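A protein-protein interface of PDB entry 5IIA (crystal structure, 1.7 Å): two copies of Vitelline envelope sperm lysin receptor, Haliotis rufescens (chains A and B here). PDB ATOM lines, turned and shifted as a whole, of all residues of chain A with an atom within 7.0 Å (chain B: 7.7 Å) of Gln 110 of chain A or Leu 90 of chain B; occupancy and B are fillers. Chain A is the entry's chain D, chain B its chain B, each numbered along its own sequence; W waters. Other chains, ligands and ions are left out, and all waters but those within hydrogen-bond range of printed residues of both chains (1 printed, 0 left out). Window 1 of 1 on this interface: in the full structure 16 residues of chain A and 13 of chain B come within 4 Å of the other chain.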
ATOM      1  N   VAL A  11      13.806   3.860  -7.928  1.00  0.00           N
ATOM      2  CA  VAL A  11      13.007   5.033  -8.282  1.00  0.00           C
ATOM      3  C   VAL A  11      12.832   5.172  -9.788  1.00  0.00           C
ATOM      4  O   VAL A  11      13.800   5.363 -10.536  1.00  0.00           O
ATOM      5  CB  VAL A  11      13.652   6.304  -7.706  1.00  0.00           C
ATOM      6  CG1 VAL A  11      12.865   7.576  -8.096  1.00  0.00           C
ATOM      7  CG2 VAL A  11      13.782   6.171  -6.199  1.00  0.00           C
ATOM      8  N   CYS A  13      11.128   7.598 -12.324  1.00  0.00           N
ATOM      9  CA  CYS A  13      10.511   8.894 -12.591  1.00  0.00           C
ATOM     10  C   CYS A  13       9.812   8.912 -13.949  1.00  0.00           C
ATOM     11  O   CYS A  13      10.231   8.207 -14.876  1.00  0.00           O
ATOM     12  CB  CYS A  13      11.577   9.993 -12.535  1.00  0.00           C
ATOM     13  SG  CYS A  13      12.592   9.997 -11.011  1.00  0.00           S
ATOM     14  N   PHE A  76       4.454  14.667  -4.915  1.00  0.00           N
ATOM     15  CA  PHE A  76       5.766  15.304  -4.862  1.00  0.00           C
ATOM     16  C   PHE A  76       5.687  16.749  -4.383  1.00  0.00           C
ATOM     17  O   PHE A  76       4.716  17.463  -4.660  1.00  0.00           O
ATOM     18  CB  PHE A  76       6.426  15.332  -6.247  1.00  0.00           C
ATOM     19  CG  PHE A  76       7.094  14.054  -6.651  1.00  0.00           C
ATOM     20  CD1 PHE A  76       8.237  13.608  -5.997  1.00  0.00           C
ATOM     21  CD2 PHE A  76       6.608  13.320  -7.718  1.00  0.00           C
ATOM     22  CE1 PHE A  76       8.879  12.458  -6.392  1.00  0.00           C
ATOM     23  CE2 PHE A  76       7.234  12.159  -8.110  1.00  0.00           C
ATOM     24  CZ  PHE A  76       8.373  11.723  -7.450  1.00  0.00           C
ATOM     25  N   LEU A  90      12.684  20.083 -10.797  1.00  0.00           N
ATOM     26  CA  LEU A  90      12.842  19.049  -9.796  1.00  0.00           C
ATOM     27  C   LEU A  90      11.543  18.824  -9.034  1.00  0.00           C
ATOM     28  O   LEU A  90      10.865  19.778  -8.621  1.00  0.00           O
ATOM     29  CB  LEU A  90      13.953  19.421  -8.802  1.00  0.00           C
ATOM     30  CG  LEU A  90      14.111  18.457  -7.614  1.00  0.00           C
ATOM     31  CD1 LEU A  90      14.655  17.110  -8.065  1.00  0.00           C
ATOM     32  CD2 LEU A  90      15.017  19.078  -6.554  1.00  0.00           C
ATOM     33  N   TYR A  91      11.208  17.545  -8.875  1.00  0.00           N
ATOM     34  CA  TYR A  91      10.183  17.094  -7.946  1.00  0.00           C
ATOM     35  C   TYR A  91      10.859  16.211  -6.901  1.00  0.00           C
ATOM     36  O   TYR A  91      11.762  15.443  -7.224  1.00  0.00           O
ATOM     37  CB  TYR A  91       9.098  16.308  -8.665  1.00  0.00           C
ATOM     38  CG  TYR A  91       8.208  17.140  -9.537  1.00  0.00           C
ATOM     39  CD1 TYR A  91       7.083  17.742  -9.013  1.00  0.00           C
ATOM     40  CD2 TYR A  91       8.485  17.315 -10.883  1.00  0.00           C
ATOM     41  CE1 TYR A  91       6.245  18.501  -9.802  1.00  0.00           C
ATOM     42  CE2 TYR A  91       7.654  18.072 -11.683  1.00  0.00           C
ATOM     43  CZ  TYR A  91       6.538  18.666 -11.130  1.00  0.00           C
ATOM     44  OH  TYR A  91       5.701  19.425 -11.910  1.00  0.00           O
ATOM     45  N   THR A  92      10.437  16.300  -5.646  1.00  0.00           N
ATOM     46  CA  THR A  92      11.125  15.537  -4.628  1.00  0.00           C
ATOM     47  C   THR A  92      10.231  15.218  -3.451  1.00  0.00           C
ATOM     48  O   THR A  92       9.233  15.900  -3.220  1.00  0.00           O
ATOM     49  CB  THR A  92      12.383  16.297  -4.130  1.00  0.00           C
ATOM     50  OG1 THR A  92      13.137  15.462  -3.250  1.00  0.00           O
ATOM     51  CG2 THR A  92      12.003  17.573  -3.398  1.00  0.00           C
ATOM     52  N   VAL A  93      10.577  14.138  -2.758  1.00  0.00           N
ATOM     53  CA  VAL A  93      10.069  13.879  -1.407  1.00  0.00           C
ATOM     54  C   VAL A  93      11.224  13.427  -0.547  1.00  0.00           C
ATOM     55  O   VAL A  93      12.274  13.027  -1.056  1.00  0.00           O
ATOM     56  CB  VAL A  93       8.938  12.797  -1.360  1.00  0.00           C
ATOM     57  CG1 VAL A  93       7.689  13.243  -2.131  1.00  0.00           C
ATOM     58  CG2 VAL A  93       9.447  11.445  -1.863  1.00  0.00           C
ATOM     59  N   THR A  94      11.026  13.463   0.764  1.00  0.00           N
ATOM     60  CA  THR A  94      11.975  12.842   1.681  1.00  0.00           C
ATOM     61  C   THR A  94      11.253  11.756   2.464  1.00  0.00           C
ATOM     62  O   THR A  94      10.030  11.786   2.605  1.00  0.00           O
ATOM     63  CB  THR A  94      12.588  13.847   2.658  1.00  0.00           C
ATOM     64  OG1 THR A  94      11.547  14.469   3.416  1.00  0.00           O
ATOM     65  CG2 THR A  94      13.391  14.900   1.905  1.00  0.00           C
ATOM     66  N   SER A 108      16.399  11.108   0.609  1.00  0.00           N
ATOM     67  CA  SER A 108      15.862  12.007  -0.400  1.00  0.00           C
ATOM     68  C   SER A 108      15.566  11.302  -1.725  1.00  0.00           C
ATOM     69  O   SER A 108      16.431  10.627  -2.292  1.00  0.00           O
ATOM     70  CB  SER A 108      16.849  13.165  -0.631  1.00  0.00           C
ATOM     71  OG  SER A 108      16.605  13.835  -1.858  1.00  0.00           O
ATOM     72  N   ILE A 109      14.329  11.437  -2.186  1.00  0.00           N
ATOM     73  CA  ILE A 109      13.914  10.926  -3.496  1.00  0.00           C
ATOM     74  C   ILE A 109      13.692  12.100  -4.452  1.00  0.00           C
ATOM     75  O   ILE A 109      12.842  12.973  -4.206  1.00  0.00           O
ATOM     76  CB  ILE A 109      12.652  10.075  -3.428  1.00  0.00           C
ATOM     77  CG1 ILE A 109      12.870   8.862  -2.529  1.00  0.00           C
ATOM     78  CG2 ILE A 109      12.261   9.605  -4.831  1.00  0.00           C
ATOM     79  CD1 ILE A 109      11.580   8.228  -2.063  1.00  0.00           C
ATOM     80  N   GLN A 110      14.494  12.129  -5.516  1.00  0.00           N
ATOM     81  CA  GLN A 110      14.456  13.209  -6.493  1.00  0.00           C
ATOM     82  C   GLN A 110      14.087  12.682  -7.873  1.00  0.00           C
ATOM     83  O   GLN A 110      14.640  11.686  -8.347  1.00  0.00           O
ATOM     84  CB  GLN A 110      15.807  13.911  -6.583  1.00  0.00           C
ATOM     85  CG  GLN A 110      16.284  14.538  -5.298  1.00  0.00           C
ATOM     86  CD  GLN A 110      17.722  14.996  -5.404  1.00  0.00           C
ATOM     87  OE1 GLN A 110      18.637  14.175  -5.492  1.00  0.00           O
ATOM     88  NE2 GLN A 110      17.933  16.310  -5.393  1.00  0.00           N
ATOM     89  N   CYS A 111      13.197  13.404  -8.533  1.00  0.00           N
ATOM     90  CA  CYS A 111      12.812  13.116  -9.902  1.00  0.00           C
ATOM     91  C   CYS A 111      12.853  14.391 -10.715  1.00  0.00           C
ATOM     92  O   CYS A 111      12.133  15.342 -10.413  1.00  0.00           O
ATOM     93  CB  CYS A 111      11.407  12.507  -9.947  1.00  0.00           C
ATOM     94  SG  CYS A 111      11.348  10.755  -9.554  1.00  0.00           S
ATOM     95  N   TYR A 112      13.666  14.398 -11.768  1.00  0.00           N
ATOM     96  CA  TYR A 112      13.722  15.541 -12.673  1.00  0.00           C
ATOM     97  C   TYR A 112      12.725  15.340 -13.804  1.00  0.00           C
ATOM     98  O   TYR A 112      12.528  14.229 -14.303  1.00  0.00           O
ATOM     99  CB  TYR A 112      15.132  15.747 -13.218  1.00  0.00           C
ATOM    100  CG  TYR A 112      16.095  16.266 -12.169  1.00  0.00           C
ATOM    101  CD1 TYR A 112      16.206  17.627 -11.919  1.00  0.00           C
ATOM    102  CD2 TYR A 112      16.865  15.400 -11.414  1.00  0.00           C
ATOM    103  CE1 TYR A 112      17.083  18.114 -10.956  1.00  0.00           C
ATOM    104  CE2 TYR A 112      17.742  15.874 -10.447  1.00  0.00           C
ATOM    105  CZ  TYR A 112      17.843  17.237 -10.223  1.00  0.00           C
ATOM    106  OH  TYR A 112      18.709  17.722  -9.265  1.00  0.00           O
ATOM    107  N   TYR B  62      26.141  23.971   6.901  1.00  0.00           N
ATOM    108  CA  TYR B  62      25.794  22.552   6.964  1.00  0.00           C
ATOM    109  C   TYR B  62      25.434  22.065   8.368  1.00  0.00           C
ATOM    110  O   TYR B  62      24.754  21.050   8.519  1.00  0.00           O
ATOM    111  CB  TYR B  62      26.956  21.721   6.437  1.00  0.00           C
ATOM    112  CG  TYR B  62      27.253  21.947   4.974  1.00  0.00           C
ATOM    113  CD1 TYR B  62      26.635  21.181   3.988  1.00  0.00           C
ATOM    114  CD2 TYR B  62      28.168  22.911   4.575  1.00  0.00           C
ATOM    115  CE1 TYR B  62      26.913  21.382   2.650  1.00  0.00           C
ATOM    116  CE2 TYR B  62      28.450  23.114   3.248  1.00  0.00           C
ATOM    117  CZ  TYR B  62      27.822  22.353   2.287  1.00  0.00           C
ATOM    118  OH  TYR B  62      28.125  22.574   0.962  1.00  0.00           O
ATOM    119  N   PHE B  76      21.262  24.295   6.066  1.00  0.00           N
ATOM    120  CA  PHE B  76      20.678  23.289   5.177  1.00  0.00           C
ATOM    121  C   PHE B  76      19.771  22.293   5.921  1.00  0.00           C
ATOM    122  O   PHE B  76      20.008  21.973   7.090  1.00  0.00           O
ATOM    123  CB  PHE B  76      21.760  22.457   4.493  1.00  0.00           C
ATOM    124  CG  PHE B  76      22.434  23.122   3.330  1.00  0.00           C
ATOM    125  CD1 PHE B  76      21.752  23.392   2.160  1.00  0.00           C
ATOM    126  CD2 PHE B  76      23.783  23.423   3.399  1.00  0.00           C
ATOM    127  CE1 PHE B  76      22.387  23.949   1.094  1.00  0.00           C
ATOM    128  CE2 PHE B  76      24.431  24.001   2.339  1.00  0.00           C
ATOM    129  CZ  PHE B  76      23.729  24.274   1.179  1.00  0.00           C
ATOM    130  N   TRP B  77      18.745  21.800   5.230  1.00  0.00           N
ATOM    131  CA  TRP B  77      18.088  20.558   5.624  1.00  0.00           C
ATOM    132  C   TRP B  77      19.021  19.412   5.269  1.00  0.00           C
ATOM    133  O   TRP B  77      19.749  19.502   4.278  1.00  0.00           O
ATOM    134  CB  TRP B  77      16.746  20.372   4.897  1.00  0.00           C
ATOM    135  CG  TRP B  77      15.685  21.365   5.235  1.00  0.00           C
ATOM    136  CD1 TRP B  77      15.349  22.473   4.527  1.00  0.00           C
ATOM    137  CD2 TRP B  77      14.797  21.326   6.364  1.00  0.00           C
ATOM    138  NE1 TRP B  77      14.315  23.139   5.144  1.00  0.00           N
ATOM    139  CE2 TRP B  77      13.956  22.454   6.269  1.00  0.00           C
ATOM    140  CE3 TRP B  77      14.638  20.457   7.442  1.00  0.00           C
ATOM    141  CZ2 TRP B  77      12.964  22.733   7.214  1.00  0.00           C
ATOM    142  CZ3 TRP B  77      13.648  20.736   8.384  1.00  0.00           C
ATOM    143  CH2 TRP B  77      12.830  21.866   8.260  1.00  0.00           C
ATOM    144  N   GLY B  78      18.927  18.302   6.002  1.00  0.00           N
ATOM    145  CA  GLY B  78      19.807  17.161   5.803  1.00  0.00           C
ATOM    146  C   GLY B  78      20.762  16.885   6.957  1.00  0.00           C
ATOM    147  O   GLY B  78      20.625  17.461   8.027  1.00  0.00           O
ATOM    148  N   PRO B  79      21.697  15.944   6.771  1.00  0.00           N
ATOM    149  CA  PRO B  79      21.999  15.236   5.525  1.00  0.00           C
ATOM    150  C   PRO B  79      20.969  14.175   5.159  1.00  0.00           C
ATOM    151  O   PRO B  79      20.357  13.569   6.034  1.00  0.00           O
ATOM    152  CB  PRO B  79      23.352  14.591   5.822  1.00  0.00           C
ATOM    153  CG  PRO B  79      23.330  14.355   7.279  1.00  0.00           C
ATOM    154  CD  PRO B  79      22.587  15.513   7.865  1.00  0.00           C
ATOM    155  N   TYR B  80      20.789  13.960   3.863  1.00  0.00           N
ATOM    156  CA  TYR B  80      19.891  12.907   3.387  1.00  0.00           C
ATOM    157  C   TYR B  80      20.690  11.865   2.643  1.00  0.00           C
ATOM    158  O   TYR B  80      21.545  12.208   1.830  1.00  0.00           O
ATOM    159  CB  TYR B  80      18.811  13.465   2.453  1.00  0.00           C
ATOM    160  CG  TYR B  80      17.860  14.446   3.067  1.00  0.00           C
ATOM    161  CD1 TYR B  80      16.804  14.027   3.855  1.00  0.00           C
ATOM    162  CD2 TYR B  80      17.996  15.808   2.825  1.00  0.00           C
ATOM    163  CE1 TYR B  80      15.923  14.941   4.407  1.00  0.00           C
ATOM    164  CE2 TYR B  80      17.139  16.710   3.360  1.00  0.00           C
ATOM    165  CZ  TYR B  80      16.107  16.284   4.155  1.00  0.00           C
ATOM    166  OH  TYR B  80      15.256  17.226   4.678  1.00  0.00           O
ATOM    167  N   SER B  81      20.370  10.594   2.874  1.00  0.00           N
ATOM    168  CA  SER B  81      20.909   9.536   2.046  1.00  0.00           C
ATOM    169  C   SER B  81      20.250   9.613   0.680  1.00  0.00           C
ATOM    170  O   SER B  81      19.076   9.950   0.554  1.00  0.00           O
ATOM    171  CB  SER B  81      20.667   8.162   2.677  1.00  0.00           C
ATOM    172  OG  SER B  81      21.294   8.068   3.943  1.00  0.00           O
ATOM    173  N   VAL B  82      21.035   9.294  -0.339  1.00  0.00           N
ATOM    174  CA  VAL B  82      20.592   9.276  -1.726  1.00  0.00           C
ATOM    175  C   VAL B  82      20.548   7.844  -2.235  1.00  0.00           C
ATOM    176  O   VAL B  82      21.507   7.109  -2.045  1.00  0.00           O
ATOM    177  CB  VAL B  82      21.548  10.122  -2.581  1.00  0.00           C
ATOM    178  CG1 VAL B  82      21.296   9.925  -4.064  1.00  0.00           C
ATOM    179  CG2 VAL B  82      21.423  11.587  -2.194  1.00  0.00           C
ATOM    180  N   PRO B  83      19.453   7.442  -2.897  1.00  0.00           N
ATOM    181  CA  PRO B  83      19.438   6.029  -3.289  1.00  0.00           C
ATOM    182  C   PRO B  83      20.520   5.707  -4.318  1.00  0.00           C
ATOM    183  O   PRO B  83      20.788   6.529  -5.194  1.00  0.00           O
ATOM    184  CB  PRO B  83      18.044   5.844  -3.901  1.00  0.00           C
ATOM    185  CG  PRO B  83      17.211   6.897  -3.276  1.00  0.00           C
ATOM    186  CD  PRO B  83      18.137   8.079  -3.086  1.00  0.00           C
ATOM    187  N   VAL B  88      27.997   9.968  -1.244  1.00  0.00           N
ATOM    188  CA  VAL B  88      27.613  11.333  -0.893  1.00  0.00           C
ATOM    189  C   VAL B  88      26.335  11.378  -0.084  1.00  0.00           C
ATOM    190  O   VAL B  88      25.580  10.410  -0.044  1.00  0.00           O
ATOM    191  CB  VAL B  88      27.436  12.204  -2.157  1.00  0.00           C
ATOM    192  CG1 VAL B  88      28.727  12.278  -2.951  1.00  0.00           C
ATOM    193  CG2 VAL B  88      26.295  11.671  -3.027  1.00  0.00           C
ATOM    194  N   VAL B  89      26.097  12.523   0.550  1.00  0.00           N
ATOM    195  CA  VAL B  89      24.804  12.804   1.150  1.00  0.00           C
ATOM    196  C   VAL B  89      24.337  14.145   0.619  1.00  0.00           C
ATOM    197  O   VAL B  89      25.143  14.932   0.130  1.00  0.00           O
ATOM    198  CB  VAL B  89      24.860  12.782   2.685  1.00  0.00           C
ATOM    199  CG1 VAL B  89      25.135  11.359   3.176  1.00  0.00           C
ATOM    200  CG2 VAL B  89      25.908  13.748   3.207  1.00  0.00           C
ATOM    201  N   LEU B  90      23.035  14.394   0.721  1.00  0.00           N
ATOM    202  CA  LEU B  90      22.427  15.597   0.177  1.00  0.00           C
ATOM    203  C   LEU B  90      22.057  16.581   1.273  1.00  0.00           C
ATOM    204  O   LEU B  90      21.447  16.230   2.264  1.00  0.00           O
ATOM    205  CB  LEU B  90      21.175  15.258  -0.645  1.00  0.00           C
ATOM    206  CG  LEU B  90      20.343  16.454  -1.179  1.00  0.00           C
ATOM    207  CD1 LEU B  90      21.096  17.219  -2.254  1.00  0.00           C
ATOM    208  CD2 LEU B  90      18.991  15.992  -1.708  1.00  0.00           C
ATOM    209  N   TYR B  91      22.424  17.835   1.054  1.00  0.00           N
ATOM    210  CA  TYR B  91      21.939  18.936   1.867  1.00  0.00           C
ATOM    211  C   TYR B  91      21.160  19.852   0.955  1.00  0.00           C
ATOM    212  O   TYR B  91      21.542  20.050  -0.190  1.00  0.00           O
ATOM    213  CB  TYR B  91      23.091  19.688   2.502  1.00  0.00           C
ATOM    214  CG  TYR B  91      23.813  18.952   3.585  1.00  0.00           C
ATOM    215  CD1 TYR B  91      23.405  19.084   4.901  1.00  0.00           C
ATOM    216  CD2 TYR B  91      24.921  18.174   3.307  1.00  0.00           C
ATOM    217  CE1 TYR B  91      24.059  18.462   5.915  1.00  0.00           C
ATOM    218  CE2 TYR B  91      25.595  17.527   4.329  1.00  0.00           C
ATOM    219  CZ  TYR B  91      25.148  17.681   5.633  1.00  0.00           C
ATOM    220  OH  TYR B  91      25.783  17.068   6.677  1.00  0.00           O
ATOM    221  N   THR B  92      20.059  20.412   1.430  1.00  0.00           N
ATOM    222  CA  THR B  92      19.276  21.259   0.543  1.00  0.00           C
ATOM    223  C   THR B  92      18.471  22.283   1.308  1.00  0.00           C
ATOM    224  O   THR B  92      18.133  22.073   2.471  1.00  0.00           O
ATOM    225  CB  THR B  92      18.326  20.408  -0.341  1.00  0.00           C
ATOM    226  OG1 THR B  92      17.673  21.254  -1.295  1.00  0.00           O
ATOM    227  CG2 THR B  92      17.284  19.660   0.503  1.00  0.00           C
ATOM    228  N   VAL B  93      18.188  23.401   0.636  1.00  0.00           N
ATOM    229  CA  VAL B  93      17.140  24.320   1.065  1.00  0.00           C
ATOM    230  C   VAL B  93      16.355  24.648  -0.191  1.00  0.00           C
ATOM    231  O   VAL B  93      16.788  24.334  -1.309  1.00  0.00           O
ATOM    232  CB  VAL B  93      17.676  25.622   1.746  1.00  0.00           C
ATOM    233  CG1 VAL B  93      18.466  25.295   3.015  1.00  0.00           C
ATOM    234  CG2 VAL B  93      18.488  26.466   0.762  1.00  0.00           C
ATOM    235  N   SER B 108      15.291  25.168  -5.907  1.00  0.00           N
ATOM    236  CA  SER B 108      15.917  24.112  -5.131  1.00  0.00           C
ATOM    237  C   SER B 108      17.414  24.367  -5.094  1.00  0.00           C
ATOM    238  O   SER B 108      18.076  24.399  -6.132  1.00  0.00           O
ATOM    239  CB  SER B 108      15.638  22.733  -5.725  1.00  0.00           C
ATOM    240  OG  SER B 108      16.552  21.776  -5.200  1.00  0.00           O
ATOM    241  N   ILE B 109      17.930  24.532  -3.882  1.00  0.00           N
ATOM    242  CA  ILE B 109      19.332  24.781  -3.648  1.00  0.00           C
ATOM    243  C   ILE B 109      19.913  23.537  -3.009  1.00  0.00           C
ATOM    244  O   ILE B 109      19.663  23.256  -1.826  1.00  0.00           O
ATOM    245  CB  ILE B 109      19.523  26.007  -2.769  1.00  0.00           C
ATOM    246  CG1 ILE B 109      18.929  27.238  -3.470  1.00  0.00           C
ATOM    247  CG2 ILE B 109      20.994  26.252  -2.482  1.00  0.00           C
ATOM    248  CD1 ILE B 109      18.618  28.379  -2.532  1.00  0.00           C
ATOM    249  N   GLN B 110      20.723  22.834  -3.795  1.00  0.00           N
ATOM    250  CA  GLN B 110      21.238  21.512  -3.425  1.00  0.00           C
ATOM    251  C   GLN B 110      22.743  21.455  -3.352  1.00  0.00           C
ATOM    252  O   GLN B 110      23.432  21.968  -4.234  1.00  0.00           O
ATOM    253  CB  GLN B 110      20.822  20.464  -4.444  1.00  0.00           C
ATOM    254  CG  GLN B 110      19.364  20.293  -4.669  1.00  0.00           C
ATOM    255  CD  GLN B 110      19.122  19.410  -5.864  1.00  0.00           C
ATOM    256  OE1 GLN B 110      19.890  18.492  -6.134  1.00  0.00           O
ATOM    257  NE2 GLN B 110      18.117  19.743  -6.640  1.00  0.00           N
ATOM    258  N   CYS B 111      23.247  20.773  -2.331  1.00  0.00           N
ATOM    259  CA  CYS B 111      24.676  20.524  -2.187  1.00  0.00           C
ATOM    260  C   CYS B 111      24.927  19.069  -1.806  1.00  0.00           C
ATOM    261  O   CYS B 111      24.334  18.571  -0.858  1.00  0.00           O
ATOM    262  CB  CYS B 111      25.281  21.463  -1.139  1.00  0.00           C
ATOM    263  SG  CYS B 111      25.574  23.135  -1.774  1.00  0.00           S
ATOM    264  N   TYR B 112      25.747  18.368  -2.582  1.00  0.00           N
ATOM    265  CA  TYR B 112      26.132  17.005  -2.219  1.00  0.00           C
ATOM    266  C   TYR B 112      27.450  17.044  -1.470  1.00  0.00           C
ATOM    267  O   TYR B 112      28.399  17.692  -1.897  1.00  0.00           O
ATOM    268  CB  TYR B 112      26.252  16.123  -3.456  1.00  0.00           C
ATOM    269  CG  TYR B 112      24.930  15.843  -4.104  1.00  0.00           C
ATOM    270  CD1 TYR B 112      24.124  14.794  -3.674  1.00  0.00           C
ATOM    271  CD2 TYR B 112      24.478  16.637  -5.146  1.00  0.00           C
ATOM    272  CE1 TYR B 112      22.906  14.547  -4.277  1.00  0.00           C
ATOM    273  CE2 TYR B 112      23.264  16.394  -5.751  1.00  0.00           C
ATOM    274  CZ  TYR B 112      22.484  15.356  -5.314  1.00  0.00           C
ATOM    275  OH  TYR B 112      21.276  15.128  -5.925  1.00  0.00           O
ATOM    276  N   MET B 113      27.500  16.344  -0.352  1.00  0.00           N
ATOM    277  CA  MET B 113      28.688  16.302   0.491  1.00  0.00           C
ATOM    278  C   MET B 113      29.269  14.890   0.439  1.00  0.00           C
ATOM    279  O   MET B 113      28.548  13.919   0.629  1.00  0.00           O
ATOM    280  CB  MET B 113      28.330  16.707   1.921  1.00  0.00           C
ATOM    281  CG  MET B 113      29.475  16.672   2.938  1.00  0.00           C
ATOM    282  SD  MET B 113      30.730  17.954   2.680  1.00  0.00           S
ATOM    283  CE  MET B 113      29.748  19.471   2.772  1.00  0.00           C
ATOM    284  N   PRO B 114      30.575  14.765   0.174  1.00  0.00           N
ATOM    285  CA  PRO B 114      31.162  13.424   0.251  1.00  0.00           C
ATOM    286  C   PRO B 114      31.060  12.849   1.655  1.00  0.00           C
ATOM    287  O   PRO B 114      31.163  13.593   2.630  1.00  0.00           O
ATOM    288  CB  PRO B 114      32.622  13.652  -0.147  1.00  0.00           C
ATOM    289  CG  PRO B 114      32.631  14.943  -0.876  1.00  0.00           C
ATOM    290  CD  PRO B 114      31.558  15.771  -0.259  1.00  0.00           C
ATOM    291  N   LYS B 115      30.818  11.546   1.756  1.00  0.00           N
ATOM    292  CA  LYS B 115      30.747  10.881   3.053  1.00  0.00           C
ATOM    293  C   LYS B 115      32.127  10.528   3.609  1.00  0.00           C
ATOM    294  O   LYS B 115      33.104  10.421   2.866  1.00  0.00           O
ATOM    295  CB  LYS B 115      29.906   9.618   2.951  1.00  0.00           C
ATOM    296  CG  LYS B 115      28.515   9.875   2.441  1.00  0.00           C
ATOM    297  CD  LYS B 115      27.640   8.643   2.557  1.00  0.00           C
ATOM    298  CE  LYS B 115      27.269   8.343   3.997  1.00  0.00           C
ATOM    299  NZ  LYS B 115      26.310   7.212   4.077  1.00  0.00           N
HETATM  300  O   HOH W   1      20.562  16.275  -8.547  1.00  0.00           O
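NE2 of Gln 110 of chain A lies within hydrogen-bond range of OE1 of Gln 110 of chain B (3.0 Å). The backbone carbonyl oxygen (O) of Ser 81 of chain B sits at hydrogen-bond distance from the backbone NH (N) of Ser 108 of chain A, at 2.9 Å. NE2 of Gln 110 of chain B is in hydrogen-bond range of OH of Tyr 112 of chain A, at 3.4 Å. The side-chain amide oxygen (OE1) of Gln 110 of chain A lies within hydrogen-bond range of the side-chain hydroxyl (OH) of Tyr 112 of chain B.
Leu 90 of chain A touches Ser 108 of chain B, and with the chains exchanged Ser 108 of chain A touches Leu 90 of chain B. Leu 90 of chain A touches Gln 110 of chain B, and with the chains exchanged Gln 110 of chain A touches Leu 90 of chain B. Gln 110 of chain B touches its own counterpart, Gln 110 of chain A. Gln 110 of chain A touches Tyr 112 of chain B, and with the chains exchanged Tyr 112 of chain A touches Gln 110 of chain B. 10 positions are printed for both chains. Of the 11 pairs that touch across the chains among the printed residues, 7 have their exchanged pair printed and touching as well.
Among the printed residues, merely in contact across the chains: Leu 90 of chain A with Ser 108 of chain B, Leu 90 of chain A with Gln 110 of chain B, Thr 94 of chain A with Tyr 80 of chain B, Ser 108 of chain A with Tyr 80 of chain B, Ser 108 of chain A with Pro 83 of chain B, Ser 108 of chain A with Leu 90 of chain B and Gln 110 of chain A with Leu 90 of chain B.
Hydrophobic or aromatic side chains of chain A that line the printed part of chain B: Leu 90 and Tyr 112. Of the 23 printed residues of chain B, 7 touch a printed residue of chain A. Among the printed residues, 11 pairs touch across the chains. Among the printed residues, no Asp or Glu carboxylate lies within 4 Å of a Lys or Arg side-chain nitrogen of the other chain.
OG of Ser 108 of chain B sits at hydrogen-bond distance from NE2 of Gln 110 of chain B, at 2.9 Å. The side-chain sulfur of Cys 13 of chain A forms a disulfide with the side-chain sulfur of Cys 111 of chain A (2.1 Å). The backbone NH of Tyr 80 of chain B lies within hydrogen-bond range of the backbone carbonyl oxygen of Leu 90 of chain B, 2.9 Å away.
Of the printed residues of chain B, Gln 110 of chain A touches Leu 90, Gln 110 and Tyr 112. Leu 90 of chain B touches just these residues of chain A: Ser 108 (3.2 Å) and Gln 110 (3.8 Å). Of the printed residues of chain A, Gln 110 of chain B touches Leu 90 (3.2 Å), Gln 110 (3.0 Å) and Tyr 112 (3.4 Å). Of the printed residues of chain A, Pro 83 of chain B touches Ser 108. Of the printed residues of chain B, Tyr 112 of chain A touches Gln 110 (3.4 Å). Of the printed residues of chain A, Ser 81 of chain B touches Ser 108. Val 93 of chain A touches none of the printed residues of chain B. The nearest residue of chain A that does not touch Leu 90 of chain B is Thr 92 of chain A (6.1 Å). The nearest printed residue of chain A that does not touch Ser 81 of chain B is Ile 109 of chain A (5.7 Å).
Water W1 lies within hydrogen-bond range of the side-chain hydroxyl of Tyr 112 of chain A (2.5 Å), the side-chain hydroxyl of Tyr 112 of chain B (2.9 Å) and the side-chain amide oxygen of Gln 110 of chain B (3.3 Å).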
